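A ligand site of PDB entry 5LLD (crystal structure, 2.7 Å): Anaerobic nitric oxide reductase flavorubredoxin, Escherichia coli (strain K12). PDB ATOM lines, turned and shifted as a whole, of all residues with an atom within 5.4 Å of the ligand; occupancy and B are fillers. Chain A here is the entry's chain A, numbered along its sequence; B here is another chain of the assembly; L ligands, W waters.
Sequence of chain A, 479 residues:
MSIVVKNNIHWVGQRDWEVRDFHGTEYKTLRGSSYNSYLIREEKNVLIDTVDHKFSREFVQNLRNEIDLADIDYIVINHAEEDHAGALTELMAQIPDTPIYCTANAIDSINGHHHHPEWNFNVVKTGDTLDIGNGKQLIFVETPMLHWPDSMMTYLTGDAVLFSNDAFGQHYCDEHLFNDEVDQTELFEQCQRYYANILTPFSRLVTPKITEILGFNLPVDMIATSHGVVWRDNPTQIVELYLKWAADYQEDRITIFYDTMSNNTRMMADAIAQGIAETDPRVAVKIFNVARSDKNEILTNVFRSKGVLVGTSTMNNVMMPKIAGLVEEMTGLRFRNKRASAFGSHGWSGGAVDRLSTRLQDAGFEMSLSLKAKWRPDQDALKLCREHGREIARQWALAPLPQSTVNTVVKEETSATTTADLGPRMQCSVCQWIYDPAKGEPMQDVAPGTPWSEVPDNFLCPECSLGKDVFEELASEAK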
ATOM      1  N   ASP A 259     -13.998  -6.767 -10.037  1.00  0.00           N
ATOM      2  CA  ASP A 259     -13.256  -5.549 -10.303  1.00  0.00           C
ATOM      3  C   ASP A 259     -12.973  -5.502 -11.789  1.00  0.00           C
ATOM      4  O   ASP A 259     -12.969  -6.537 -12.458  1.00  0.00           O
ATOM      5  CB  ASP A 259     -11.964  -5.503  -9.487  1.00  0.00           C
ATOM      6  CG  ASP A 259     -11.522  -4.072  -9.192  1.00  0.00           C
ATOM      7  OD1 ASP A 259     -11.818  -3.175  -9.998  1.00  0.00           O
ATOM      8  OD2 ASP A 259     -10.883  -3.861  -8.141  1.00  0.00           O
ATOM      9  N   THR A 260     -12.741  -4.303 -12.324  1.00  0.00           N
ATOM     10  CA  THR A 260     -12.576  -4.155 -13.768  1.00  0.00           C
ATOM     11  C   THR A 260     -11.721  -2.939 -14.118  1.00  0.00           C
ATOM     12  O   THR A 260     -11.738  -1.919 -13.414  1.00  0.00           O
ATOM     13  CB  THR A 260     -13.956  -4.048 -14.468  1.00  0.00           C
ATOM     14  OG1 THR A 260     -13.768  -3.992 -15.885  1.00  0.00           O
ATOM     15  CG2 THR A 260     -14.709  -2.820 -13.995  1.00  0.00           C
ATOM     16  N   MET A 261     -10.963  -3.051 -15.206  1.00  0.00           N
ATOM     17  CA  MET A 261     -10.092  -1.974 -15.641  1.00  0.00           C
ATOM     18  C   MET A 261     -10.700  -1.162 -16.793  1.00  0.00           C
ATOM     19  O   MET A 261     -10.489   0.047 -16.886  1.00  0.00           O
ATOM     20  CB  MET A 261      -8.722  -2.523 -16.054  1.00  0.00           C
ATOM     21  CG  MET A 261      -7.907  -3.062 -14.893  1.00  0.00           C
ATOM     22  SD  MET A 261      -6.316  -3.732 -15.419  1.00  0.00           S
ATOM     23  CE  MET A 261      -6.843  -5.066 -16.481  1.00  0.00           C
ATOM     24  N   SER A 262     -11.458  -1.830 -17.657  1.00  0.00           N
ATOM     25  CA  SER A 262     -12.085  -1.156 -18.790  1.00  0.00           C
ATOM     26  C   SER A 262     -13.566  -1.528 -18.963  1.00  0.00           C
ATOM     27  O   SER A 262     -14.128  -1.368 -20.043  1.00  0.00           O
ATOM     28  CB  SER A 262     -11.303  -1.416 -20.080  1.00  0.00           C
ATOM     29  OG  SER A 262     -10.995  -2.791 -20.247  1.00  0.00           O
ATOM     30  N   ASN A 263     -14.176  -2.017 -17.885  1.00  0.00           N
ATOM     31  CA  ASN A 263     -15.610  -2.282 -17.845  1.00  0.00           C
ATOM     32  C   ASN A 263     -16.083  -3.505 -18.634  1.00  0.00           C
ATOM     33  O   ASN A 263     -17.283  -3.689 -18.819  1.00  0.00           O
ATOM     34  CB  ASN A 263     -16.410  -1.052 -18.284  1.00  0.00           C
ATOM     35  CG  ASN A 263     -16.431   0.040 -17.227  1.00  0.00           C
ATOM     36  OD1 ASN A 263     -16.308  -0.239 -16.030  1.00  0.00           O
ATOM     37  ND2 ASN A 263     -16.594   1.285 -17.661  1.00  0.00           N
ATOM     38  N   ASN A 264     -15.151  -4.334 -19.083  1.00  0.00           N
ATOM     39  CA  ASN A 264     -15.508  -5.551 -19.801  1.00  0.00           C
ATOM     40  C   ASN A 264     -16.169  -6.578 -18.876  1.00  0.00           C
ATOM     41  O   ASN A 264     -17.196  -7.162 -19.216  1.00  0.00           O
ATOM     42  CB  ASN A 264     -14.292  -6.154 -20.501  1.00  0.00           C
ATOM     43  CG  ASN A 264     -13.820  -5.317 -21.682  1.00  0.00           C
ATOM     44  OD1 ASN A 264     -14.611  -4.606 -22.301  1.00  0.00           O
ATOM     45  ND2 ASN A 264     -12.530  -5.400 -21.986  1.00  0.00           N
ATOM     46  N   THR A 265     -15.561  -6.791 -17.714  1.00  0.00           N
ATOM     47  CA  THR A 265     -16.081  -7.715 -16.727  1.00  0.00           C
ATOM     48  C   THR A 265     -17.404  -7.205 -16.161  1.00  0.00           C
ATOM     49  O   THR A 265     -18.252  -7.980 -15.717  1.00  0.00           O
ATOM     50  CB  THR A 265     -15.080  -7.939 -15.584  1.00  0.00           C
ATOM     51  OG1 THR A 265     -13.866  -8.471 -16.108  1.00  0.00           O
ATOM     52  CG2 THR A 265     -15.643  -8.893 -14.542  1.00  0.00           C
ATOM     53  N   ARG A 266     -17.561  -5.884 -16.171  1.00  0.00           N
ATOM     54  CA  ARG A 266     -18.802  -5.271 -15.714  1.00  0.00           C
ATOM     55  C   ARG A 266     -19.958  -5.668 -16.624  1.00  0.00           C
ATOM     56  O   ARG A 266     -21.046  -6.001 -16.172  1.00  0.00           O
ATOM     57  CB  ARG A 266     -18.684  -3.747 -15.692  1.00  0.00           C
ATOM     58  CG  ARG A 266     -19.987  -3.042 -15.364  1.00  0.00           C
ATOM     59  CD  ARG A 266     -19.857  -1.542 -15.543  1.00  0.00           C
ATOM     60  NE  ARG A 266     -21.075  -0.854 -15.125  1.00  0.00           N
ATOM     61  CZ  ARG A 266     -21.232   0.466 -15.135  1.00  0.00           C
ATOM     62  NH1 ARG A 266     -20.246   1.253 -15.546  1.00  0.00           N
ATOM     63  NH2 ARG A 266     -22.379   1.000 -14.745  1.00  0.00           N
ATOM     64  N   SER A 313     -10.694  -9.530 -14.269  1.00  0.00           N
ATOM     65  CA  SER A 313      -9.952  -9.669 -15.509  1.00  0.00           C
ATOM     66  C   SER A 313      -8.542 -10.126 -15.164  1.00  0.00           C
ATOM     67  O   SER A 313      -8.151 -10.134 -13.997  1.00  0.00           O
ATOM     68  CB  SER A 313      -9.901  -8.334 -16.245  1.00  0.00           C
ATOM     69  OG  SER A 313      -9.259  -7.350 -15.458  1.00  0.00           O
ATOM     70  N   THR A 314      -7.767 -10.491 -16.190  1.00  0.00           N
ATOM     71  CA  THR A 314      -6.376 -10.851 -15.968  1.00  0.00           C
ATOM     72  C   THR A 314      -5.492  -9.613 -16.045  1.00  0.00           C
ATOM     73  O   THR A 314      -5.570  -8.849 -17.004  1.00  0.00           O
ATOM     74  CB  THR A 314      -5.883 -11.902 -16.984  1.00  0.00           C
ATOM     75  OG1 THR A 314      -6.569 -13.141 -16.765  1.00  0.00           O
ATOM     76  CG2 THR A 314      -4.391 -12.119 -16.824  1.00  0.00           C
ATOM     77  N   MET A 315      -4.649  -9.435 -15.031  1.00  0.00           N
ATOM     78  CA  MET A 315      -3.731  -8.316 -14.991  1.00  0.00           C
ATOM     79  C   MET A 315      -2.340  -8.807 -14.579  1.00  0.00           C
ATOM     80  O   MET A 315      -2.142  -9.223 -13.442  1.00  0.00           O
ATOM     81  CB  MET A 315      -4.217  -7.248 -13.998  1.00  0.00           C
ATOM     82  CG  MET A 315      -3.386  -5.985 -13.978  1.00  0.00           C
ATOM     83  SD  MET A 315      -3.686  -4.977 -12.517  1.00  0.00           S
ATOM     84  CE  MET A 315      -3.109  -6.080 -11.226  1.00  0.00           C
ATOM     85  N   ASN A 316      -1.409  -8.764 -15.521  1.00  0.00           N
ATOM     86  CA  ASN A 316      -0.049  -9.239 -15.267  1.00  0.00           C
ATOM     87  C   ASN A 316      -0.013 -10.699 -14.855  1.00  0.00           C
ATOM     88  O   ASN A 316       0.708 -11.077 -13.941  1.00  0.00           O
ATOM     89  CB  ASN A 316       0.649  -8.369 -14.213  1.00  0.00           C
ATOM     90  CG  ASN A 316       0.766  -6.913 -14.638  1.00  0.00           C
ATOM     91  OD1 ASN A 316       0.926  -6.605 -15.823  1.00  0.00           O
ATOM     92  ND2 ASN A 316       0.699  -6.011 -13.667  1.00  0.00           N
ATOM     93  N   ASN A 317      -0.809 -11.522 -15.538  1.00  0.00           N
ATOM     94  CA  ASN A 317      -0.850 -12.960 -15.302  1.00  0.00           C
ATOM     95  C   ASN A 317      -1.487 -13.348 -13.969  1.00  0.00           C
ATOM     96  O   ASN A 317      -1.473 -14.523 -13.587  1.00  0.00           O
ATOM     97  CB  ASN A 317       0.547 -13.565 -15.399  1.00  0.00           C
ATOM     98  CG  ASN A 317       1.195 -13.322 -16.754  1.00  0.00           C
ATOM     99  OD1 ASN A 317       2.272 -12.721 -16.844  1.00  0.00           O
ATOM    100  ND2 ASN A 317       0.534 -13.773 -17.815  1.00  0.00           N
ATOM    101  N   VAL A 318      -2.059 -12.376 -13.262  1.00  0.00           N
ATOM    102  CA  VAL A 318      -2.663 -12.639 -11.961  1.00  0.00           C
ATOM    103  C   VAL A 318      -4.034 -11.987 -11.841  1.00  0.00           C
ATOM    104  O   VAL A 318      -4.499 -11.315 -12.772  1.00  0.00           O
ATOM    105  CB  VAL A 318      -1.770 -12.147 -10.811  1.00  0.00           C
ATOM    106  CG1 VAL A 318      -0.415 -12.842 -10.852  1.00  0.00           C
ATOM    107  CG2 VAL A 318      -1.595 -10.637 -10.878  1.00  0.00           C
ATOM    108  N   MET A 320      -6.868  -9.362  -9.998  1.00  0.00           N
ATOM    109  CA  MET A 320      -6.791  -7.961  -9.599  1.00  0.00           C
ATOM    110  C   MET A 320      -6.687  -7.893  -8.080  1.00  0.00           C
ATOM    111  O   MET A 320      -7.334  -8.662  -7.371  1.00  0.00           O
ATOM    112  CB  MET A 320      -8.015  -7.198 -10.106  1.00  0.00           C
ATOM    113  CG  MET A 320      -8.183  -7.286 -11.616  1.00  0.00           C
ATOM    114  SD  MET A 320      -9.087  -5.893 -12.299  1.00  0.00           S
ATOM    115  CE  MET A 320      -8.098  -4.537 -11.701  1.00  0.00           C
ATOM    116  N   SER A 345     -12.943 -11.315 -18.025  1.00  0.00           N
ATOM    117  CA  SER A 345     -12.406 -11.125 -19.368  1.00  0.00           C
ATOM    118  C   SER A 345     -10.889 -11.162 -19.343  1.00  0.00           C
ATOM    119  O   SER A 345     -10.270 -11.099 -18.273  1.00  0.00           O
ATOM    120  CB  SER A 345     -12.888  -9.790 -19.941  1.00  0.00           C
ATOM    121  OG  SER A 345     -12.352  -9.567 -21.232  1.00  0.00           O
ATOM    122  N   HIS A 346     -10.270 -11.269 -20.516  1.00  0.00           N
ATOM    123  CA  HIS A 346      -8.818 -11.294 -20.619  1.00  0.00           C
ATOM    124  C   HIS A 346      -8.398 -10.836 -22.016  1.00  0.00           C
ATOM    125  O   HIS A 346      -9.235 -10.734 -22.913  1.00  0.00           O
ATOM    126  CB  HIS A 346      -8.286 -12.696 -20.350  1.00  0.00           C
ATOM    127  CG  HIS A 346      -8.619 -13.694 -21.412  1.00  0.00           C
ATOM    128  ND1 HIS A 346      -9.841 -14.333 -21.477  1.00  0.00           N
ATOM    129  CD2 HIS A 346      -7.899 -14.153 -22.462  1.00  0.00           C
ATOM    130  CE1 HIS A 346      -9.853 -15.146 -22.520  1.00  0.00           C
ATOM    131  NE2 HIS A 346      -8.682 -15.058 -23.126  1.00  0.00           N
ATOM    132  N   GLY A 347      -7.106 -10.578 -22.182  1.00  0.00           N
ATOM    133  CA  GLY A 347      -6.619 -10.030 -23.434  1.00  0.00           C
ATOM    134  C   GLY A 347      -5.952 -11.049 -24.334  1.00  0.00           C
ATOM    135  O   GLY A 347      -6.210 -11.064 -25.539  1.00  0.00           O
ATOM    136  N   TRP A 348      -5.091 -11.876 -23.774  1.00  0.00           N
ATOM    137  CA  TRP A 348      -4.391 -12.892 -24.558  1.00  0.00           C
ATOM    138  C   TRP A 348      -4.306 -14.250 -23.850  1.00  0.00           C
ATOM    139  O   TRP A 348      -5.089 -15.152 -24.141  1.00  0.00           O
ATOM    140  CB  TRP A 348      -3.002 -12.390 -24.975  1.00  0.00           C
ATOM    141  CG  TRP A 348      -2.214 -11.724 -23.891  1.00  0.00           C
ATOM    142  CD1 TRP A 348      -1.219 -12.284 -23.125  1.00  0.00           C
ATOM    143  CD2 TRP A 348      -2.322 -10.353 -23.459  1.00  0.00           C
ATOM    144  NE1 TRP A 348      -0.726 -11.352 -22.243  1.00  0.00           N
ATOM    145  CE2 TRP A 348      -1.379 -10.170 -22.432  1.00  0.00           C
ATOM    146  CE3 TRP A 348      -3.134  -9.280 -23.850  1.00  0.00           C
ATOM    147  CZ2 TRP A 348      -1.229  -8.946 -21.779  1.00  0.00           C
ATOM    148  CZ3 TRP A 348      -2.976  -8.068 -23.200  1.00  0.00           C
ATOM    149  CH2 TRP A 348      -2.036  -7.905 -22.171  1.00  0.00           C
ATOM    150  N   SER A 349      -3.361 -14.387 -22.922  1.00  0.00           N
ATOM    151  CA  SER A 349      -3.135 -15.667 -22.245  1.00  0.00           C
ATOM    152  C   SER A 349      -4.135 -15.921 -21.122  1.00  0.00           C
ATOM    153  O   SER A 349      -4.497 -17.075 -20.852  1.00  0.00           O
ATOM    154  CB  SER A 349      -1.710 -15.739 -21.704  1.00  0.00           C
ATOM    155  OG  SER A 349      -1.500 -14.766 -20.690  1.00  0.00           O
ATOM    156  N   GLY A 350      -4.589 -14.858 -20.461  1.00  0.00           N
ATOM    157  CA  GLY A 350      -5.531 -14.971 -19.368  1.00  0.00           C
ATOM    158  C   GLY A 350      -4.974 -15.753 -18.192  1.00  0.00           C
ATOM    159  O   GLY A 350      -3.761 -15.762 -17.956  1.00  0.00           O
ATOM    160  N   LYS A 374     -13.254 -12.853 -24.160  1.00  0.00           N
ATOM    161  CA  LYS A 374     -12.055 -12.163 -24.619  1.00  0.00           C
ATOM    162  C   LYS A 374     -12.384 -10.716 -24.978  1.00  0.00           C
ATOM    163  O   LYS A 374     -13.344 -10.462 -25.696  1.00  0.00           O
ATOM    164  CB  LYS A 374     -11.444 -12.888 -25.820  1.00  0.00           C
ATOM    165  CG  LYS A 374     -10.045 -12.415 -26.187  1.00  0.00           C
ATOM    166  CD  LYS A 374      -9.501 -13.179 -27.379  1.00  0.00           C
ATOM    167  CE  LYS A 374      -8.045 -12.821 -27.656  1.00  0.00           C
ATOM    168  NZ  LYS A 374      -7.476 -13.596 -28.792  1.00  0.00           N
ATOM    169  N   TRP A 375     -11.587  -9.792 -24.463  1.00  0.00           N
ATOM    170  CA  TRP A 375     -11.834  -8.369 -24.668  1.00  0.00           C
ATOM    171  C   TRP A 375     -13.276  -8.006 -24.325  1.00  0.00           C
ATOM    172  O   TRP A 375     -13.847  -8.549 -23.372  1.00  0.00           O
ATOM    173  CB  TRP A 375     -11.486  -7.954 -26.107  1.00  0.00           C
ATOM    174  CG  TRP A 375     -10.081  -8.305 -26.512  1.00  0.00           C
ATOM    175  CD1 TRP A 375      -9.710  -9.259 -27.422  1.00  0.00           C
ATOM    176  CD2 TRP A 375      -8.865  -7.720 -26.028  1.00  0.00           C
ATOM    177  NE1 TRP A 375      -8.347  -9.301 -27.530  1.00  0.00           N
ATOM    178  CE2 TRP A 375      -7.802  -8.369 -26.684  1.00  0.00           C
ATOM    179  CE3 TRP A 375      -8.579  -6.713 -25.098  1.00  0.00           C
ATOM    180  CZ2 TRP A 375      -6.466  -8.041 -26.437  1.00  0.00           C
ATOM    181  CZ3 TRP A 375      -7.254  -6.383 -24.859  1.00  0.00           C
ATOM    182  CH2 TRP A 375      -6.219  -7.049 -25.527  1.00  0.00           C
ATOM    183  N   ARG A 376     -13.859  -7.082 -25.081  1.00  0.00           N
ATOM    184  CA  ARG A 376     -15.224  -6.634 -24.814  1.00  0.00           C
ATOM    185  C   ARG A 376     -16.253  -7.560 -25.439  1.00  0.00           C
ATOM    186  O   ARG A 376     -16.235  -7.800 -26.646  1.00  0.00           O
ATOM    187  CB  ARG A 376     -15.423  -5.207 -25.334  1.00  0.00           C
ATOM    188  CG  ARG A 376     -16.783  -4.613 -24.988  1.00  0.00           C
ATOM    189  CD  ARG A 376     -17.094  -3.415 -25.878  1.00  0.00           C
ATOM    190  NE  ARG A 376     -15.958  -2.510 -25.980  1.00  0.00           N
ATOM    191  CZ  ARG A 376     -15.792  -1.425 -25.226  1.00  0.00           C
ATOM    192  NH1 ARG A 376     -16.690  -1.109 -24.309  1.00  0.00           N
ATOM    193  NH2 ARG A 376     -14.720  -0.656 -25.400  1.00  0.00           N
ATOM    194  N   HIS B  23      -7.036   2.258 -15.386  1.00  0.00           N
ATOM    195  CA  HIS B  23      -7.182   0.825 -15.151  1.00  0.00           C
ATOM    196  C   HIS B  23      -8.057   0.578 -13.929  1.00  0.00           C
ATOM    197  O   HIS B  23      -7.634  -0.075 -12.967  1.00  0.00           O
ATOM    198  CB  HIS B  23      -5.809   0.183 -14.939  1.00  0.00           C
ATOM    199  CG  HIS B  23      -4.886   0.314 -16.110  1.00  0.00           C
ATOM    200  ND1 HIS B  23      -3.526   0.134 -15.996  1.00  0.00           N
ATOM    201  CD2 HIS B  23      -5.131   0.595 -17.407  1.00  0.00           C
ATOM    202  CE1 HIS B  23      -2.967   0.310 -17.178  1.00  0.00           C
ATOM    203  NE2 HIS B  23      -3.924   0.594 -18.054  1.00  0.00           N
ATOM    204  N   GLU B  81      -5.578   0.214 -26.957  1.00  0.00           N
ATOM    205  CA  GLU B  81      -6.193   0.429 -25.651  1.00  0.00           C
ATOM    206  C   GLU B  81      -7.130   1.643 -25.708  1.00  0.00           C
ATOM    207  O   GLU B  81      -6.883   2.593 -26.451  1.00  0.00           O
ATOM    208  CB  GLU B  81      -5.132   0.588 -24.563  1.00  0.00           C
ATOM    209  CG  GLU B  81      -5.671   0.454 -23.148  1.00  0.00           C
ATOM    210  CD  GLU B  81      -4.572   0.249 -22.117  1.00  0.00           C
ATOM    211  OE1 GLU B  81      -3.455  -0.139 -22.512  1.00  0.00           O
ATOM    212  OE2 GLU B  81      -4.837   0.465 -20.911  1.00  0.00           O
ATOM    213  N   HIS B 113     -12.549  -4.715 -29.285  1.00  0.00           N
ATOM    214  CA  HIS B 113     -13.071  -3.502 -28.659  1.00  0.00           C
ATOM    215  C   HIS B 113     -14.200  -2.862 -29.461  1.00  0.00           C
ATOM    216  O   HIS B 113     -15.197  -2.402 -28.904  1.00  0.00           O
ATOM    217  CB  HIS B 113     -11.956  -2.464 -28.466  1.00  0.00           C
ATOM    218  CG  HIS B 113     -11.040  -2.766 -27.318  1.00  0.00           C
ATOM    219  ND1 HIS B 113     -10.335  -3.941 -27.206  1.00  0.00           N
ATOM    220  CD2 HIS B 113     -10.702  -2.020 -26.232  1.00  0.00           C
ATOM    221  CE1 HIS B 113      -9.619  -3.921 -26.101  1.00  0.00           C
ATOM    222  NE2 HIS B 113      -9.820  -2.768 -25.492  1.00  0.00           N
ATOM    223  N   HIS B 147       3.416  -2.078 -23.971  1.00  0.00           N
ATOM    224  CA  HIS B 147       3.151  -3.046 -22.910  1.00  0.00           C
ATOM    225  C   HIS B 147       2.142  -4.122 -23.299  1.00  0.00           C
ATOM    226  O   HIS B 147       1.880  -5.037 -22.521  1.00  0.00           O
ATOM    227  CB  HIS B 147       2.672  -2.318 -21.653  1.00  0.00           C
ATOM    228  CG  HIS B 147       1.434  -1.503 -21.866  1.00  0.00           C
ATOM    229  ND1 HIS B 147       0.207  -1.851 -21.342  1.00  0.00           N
ATOM    230  CD2 HIS B 147       1.228  -0.349 -22.546  1.00  0.00           C
ATOM    231  CE1 HIS B 147      -0.700  -0.964 -21.692  1.00  0.00           C
ATOM    232  NE2 HIS B 147      -0.105  -0.036 -22.420  1.00  0.00           N
ATOM    233  N   TRP B 148       1.560  -4.006 -24.498  1.00  0.00           N
ATOM    234  CA  TRP B 148       0.586  -5.001 -24.960  1.00  0.00           C
ATOM    235  C   TRP B 148       1.127  -5.767 -26.162  1.00  0.00           C
ATOM    236  O   TRP B 148       2.009  -5.286 -26.870  1.00  0.00           O
ATOM    237  CB  TRP B 148      -0.743  -4.335 -25.332  1.00  0.00           C
ATOM    238  CG  TRP B 148      -1.687  -4.181 -24.181  1.00  0.00           C
ATOM    239  CD1 TRP B 148      -1.401  -4.335 -22.855  1.00  0.00           C
ATOM    240  CD2 TRP B 148      -3.084  -3.851 -24.256  1.00  0.00           C
ATOM    241  NE1 TRP B 148      -2.532  -4.126 -22.099  1.00  0.00           N
ATOM    242  CE2 TRP B 148      -3.577  -3.815 -22.930  1.00  0.00           C
ATOM    243  CE3 TRP B 148      -3.965  -3.569 -25.309  1.00  0.00           C
ATOM    244  CZ2 TRP B 148      -4.908  -3.523 -22.638  1.00  0.00           C
ATOM    245  CZ3 TRP B 148      -5.284  -3.278 -25.010  1.00  0.00           C
ATOM    246  CH2 TRP B 148      -5.738  -3.258 -23.685  1.00  0.00           C
HETATM  247  N1  LIG L   1      -4.577 -10.003 -20.585  1.00  0.00           N
HETATM  248  C1  LIG L   1      -4.067 -11.280 -20.468  1.00  0.00           C
HETATM  249  O1  LIG L   1      -4.559 -12.197 -21.101  1.00  0.00           O
HETATM  250  N2  LIG L   1      -2.988 -11.515 -19.638  1.00  0.00           N
HETATM  251  C2  LIG L   1      -2.418 -10.482 -18.915  1.00  0.00           C
HETATM  252  O2  LIG L   1      -1.456 -10.695 -18.177  1.00  0.00           O
HETATM  253  C3  LIG L   1      -2.937  -9.194 -19.030  1.00  0.00           C
HETATM  254  N3  LIG L   1      -2.382  -8.161 -18.323  1.00  0.00           N
HETATM  255  C4  LIG L   1      -2.912  -6.881 -18.434  1.00  0.00           C
HETATM  256  C5  LIG L   1      -2.344  -5.839 -17.721  1.00  0.00           C
HETATM  257  C6  LIG L   1      -2.874  -4.559 -17.833  1.00  0.00           C
HETATM  258  C7  LIG L   1      -2.261  -3.428 -17.051  1.00  0.00           C
HETATM  259  C8  LIG L   1      -3.951  -4.314 -18.663  1.00  0.00           C
HETATM  260  C9  LIG L   1      -4.510  -2.929 -18.789  1.00  0.00           C
HETATM  261  C10 LIG L   1      -4.514  -5.368 -19.388  1.00  0.00           C
HETATM  262  C11 LIG L   1      -3.996  -6.656 -19.273  1.00  0.00           C
HETATM  263  N4  LIG L   1      -4.554  -7.700 -19.989  1.00  0.00           N
HETATM  264  C12 LIG L   1      -4.030  -8.968 -19.866  1.00  0.00           C
HETATM  265  C13 LIG L   1      -5.719  -7.467 -20.898  1.00  0.00           C
HETATM  266  C14 LIG L   1      -7.045  -7.410 -20.146  1.00  0.00           C
HETATM  267  O3  LIG L   1      -7.206  -8.575 -19.382  1.00  0.00           O
HETATM  268  C15 LIG L   1      -8.190  -7.287 -21.142  1.00  0.00           C
HETATM  269  O4  LIG L   1      -8.145  -5.990 -21.689  1.00  0.00           O
HETATM  270  C16 LIG L   1      -9.538  -7.517 -20.482  1.00  0.00           C
HETATM  271  O5  LIG L   1     -10.517  -7.652 -21.480  1.00  0.00           O
HETATM  272  C17 LIG L   1      -9.920  -6.350 -19.594  1.00  0.00           C
HETATM  273  O6  LIG L   1     -10.942  -6.767 -18.712  1.00  0.00           O
HETATM  274  P1  LIG L   1     -11.727  -5.680 -17.821  1.00  0.00           P
HETATM  275  O7  LIG L   1     -13.027  -6.275 -17.366  1.00  0.00           O
HETATM  276  O8  LIG L   1     -10.883  -5.309 -16.623  1.00  0.00           O
HETATM  277  O9  LIG L   1     -12.005  -4.453 -18.648  1.00  0.00           O
HETATM  278  O   HOH W   1     -10.059  -4.168 -22.517  1.00  0.00           O
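Water W1 lies within hydrogen-bond range of O4 of the ligand (2.8 Å), ND2 of Asn 264 (2.8 Å), OG of Ser 262 (2.8 Å) and NE2 of His 113 of chain B (3.3 Å).
Residues that only touch the ligand: Met 315 (3.6 Å), His 346 (3.4 Å), Trp 375 (3.3 Å), His 23 of chain B (3.6 Å) and Trp 148 of chain B (3.6 Å). 20 residues have an atom within 4 Å of the ligand: Thr 260, Met 261, Ser 262, Asn 263, Asn 264, Thr 265, Ser 313, Thr 314, Met 315, Asn 316, Asn 317, Ser 345, His 346, Gly 347, Trp 348, Ser 349, Gly 350, Trp 375, His 23 of chain B and Trp 148 of chain B. Along chain A the residues within 4 Å of the ligand span positions 260 to 375.
A ring nitrogen (NE2) of His 23 of chain B lies within hydrogen-bond range of the side-chain carboxylate (OE2) of Glu 81 of chain B (3.0 Å). OG1 of Thr 260 sits at hydrogen-bond distance from N of Asn 263, at 2.8 Å. The backbone carbonyl oxygen (O) of Trp 375 sits at hydrogen-bond distance from the side-chain hydroxyl (OG) of Ser 345, 2.8 Å away. The backbone carbonyl oxygen of His 346 sits at hydrogen-bond distance from the backbone NH of Trp 375 (3.0 Å). OG of Ser 262 is in hydrogen-bond range of ND2 of Asn 264. The backbone carbonyl oxygen (O) of Ser 345 lies within hydrogen-bond range of the backbone NH (N) of Thr 314 (3.3 Å). O of Gly 347 lies close to NE1 of Trp 375 (3.4 Å). OG of Ser 313 is in hydrogen-bond range of SD of Met 320 (3.5 Å).
The side-chain hydroxyl (OG) of Ser 262 is in hydrogen-bond range of an oxygen (O9) of the ligand. An oxygen (O1) of the ligand is in hydrogen-bond range of the backbone NH (N) of Ser 349 (3.1 Å). N of Gly 347 lies within hydrogen-bond range of N1 of the ligand. OG of Ser 313 lies within hydrogen-bond range of O8 of the ligand. An oxygen (O3) of the ligand lies within hydrogen-bond range of the backbone carbonyl oxygen (O) of Thr 314 (2.9 Å). The backbone NH (N) of Ser 262 lies within hydrogen-bond range of an oxygen (O9) of the ligand, at 2.9 Å. O9 of the ligand sits at hydrogen-bond distance from N of Asn 264 (3.2 Å). An oxygen (O7) of the ligand lies within hydrogen-bond range of the side-chain hydroxyl (OG1) of Thr 265 (2.7 Å). O9 of the ligand lies within hydrogen-bond range of N of Asn 263 (3.4 Å). An oxygen (O1) of the ligand lies within hydrogen-bond range of the backbone NH (N) of Trp 348 (2.7 Å). O5 of the ligand is in hydrogen-bond range of OG of Ser 345 (2.7 Å). OG1 of Thr 260 sits at hydrogen-bond distance from O7 of the ligand. An oxygen (O1) of the ligand is in hydrogen-bond range of the backbone NH of Gly 350 (2.7 Å). An oxygen (O8) of the ligand lies within hydrogen-bond range of the backbone NH of Met 261. O2 of the ligand sits at hydrogen-bond distance from N of Asn 317, at 2.8 Å. A nitrogen (N3) of the ligand lies within hydrogen-bond range of the backbone NH of Asn 316, 3.0 Å away. The backbone NH of Thr 265 is in hydrogen-bond range of an oxygen (O7) of the ligand. The side-chain amide nitrogen (ND2) of Asn 264 is in hydrogen-bond range of an oxygen (O5) of the ligand, 3.1 Å away.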
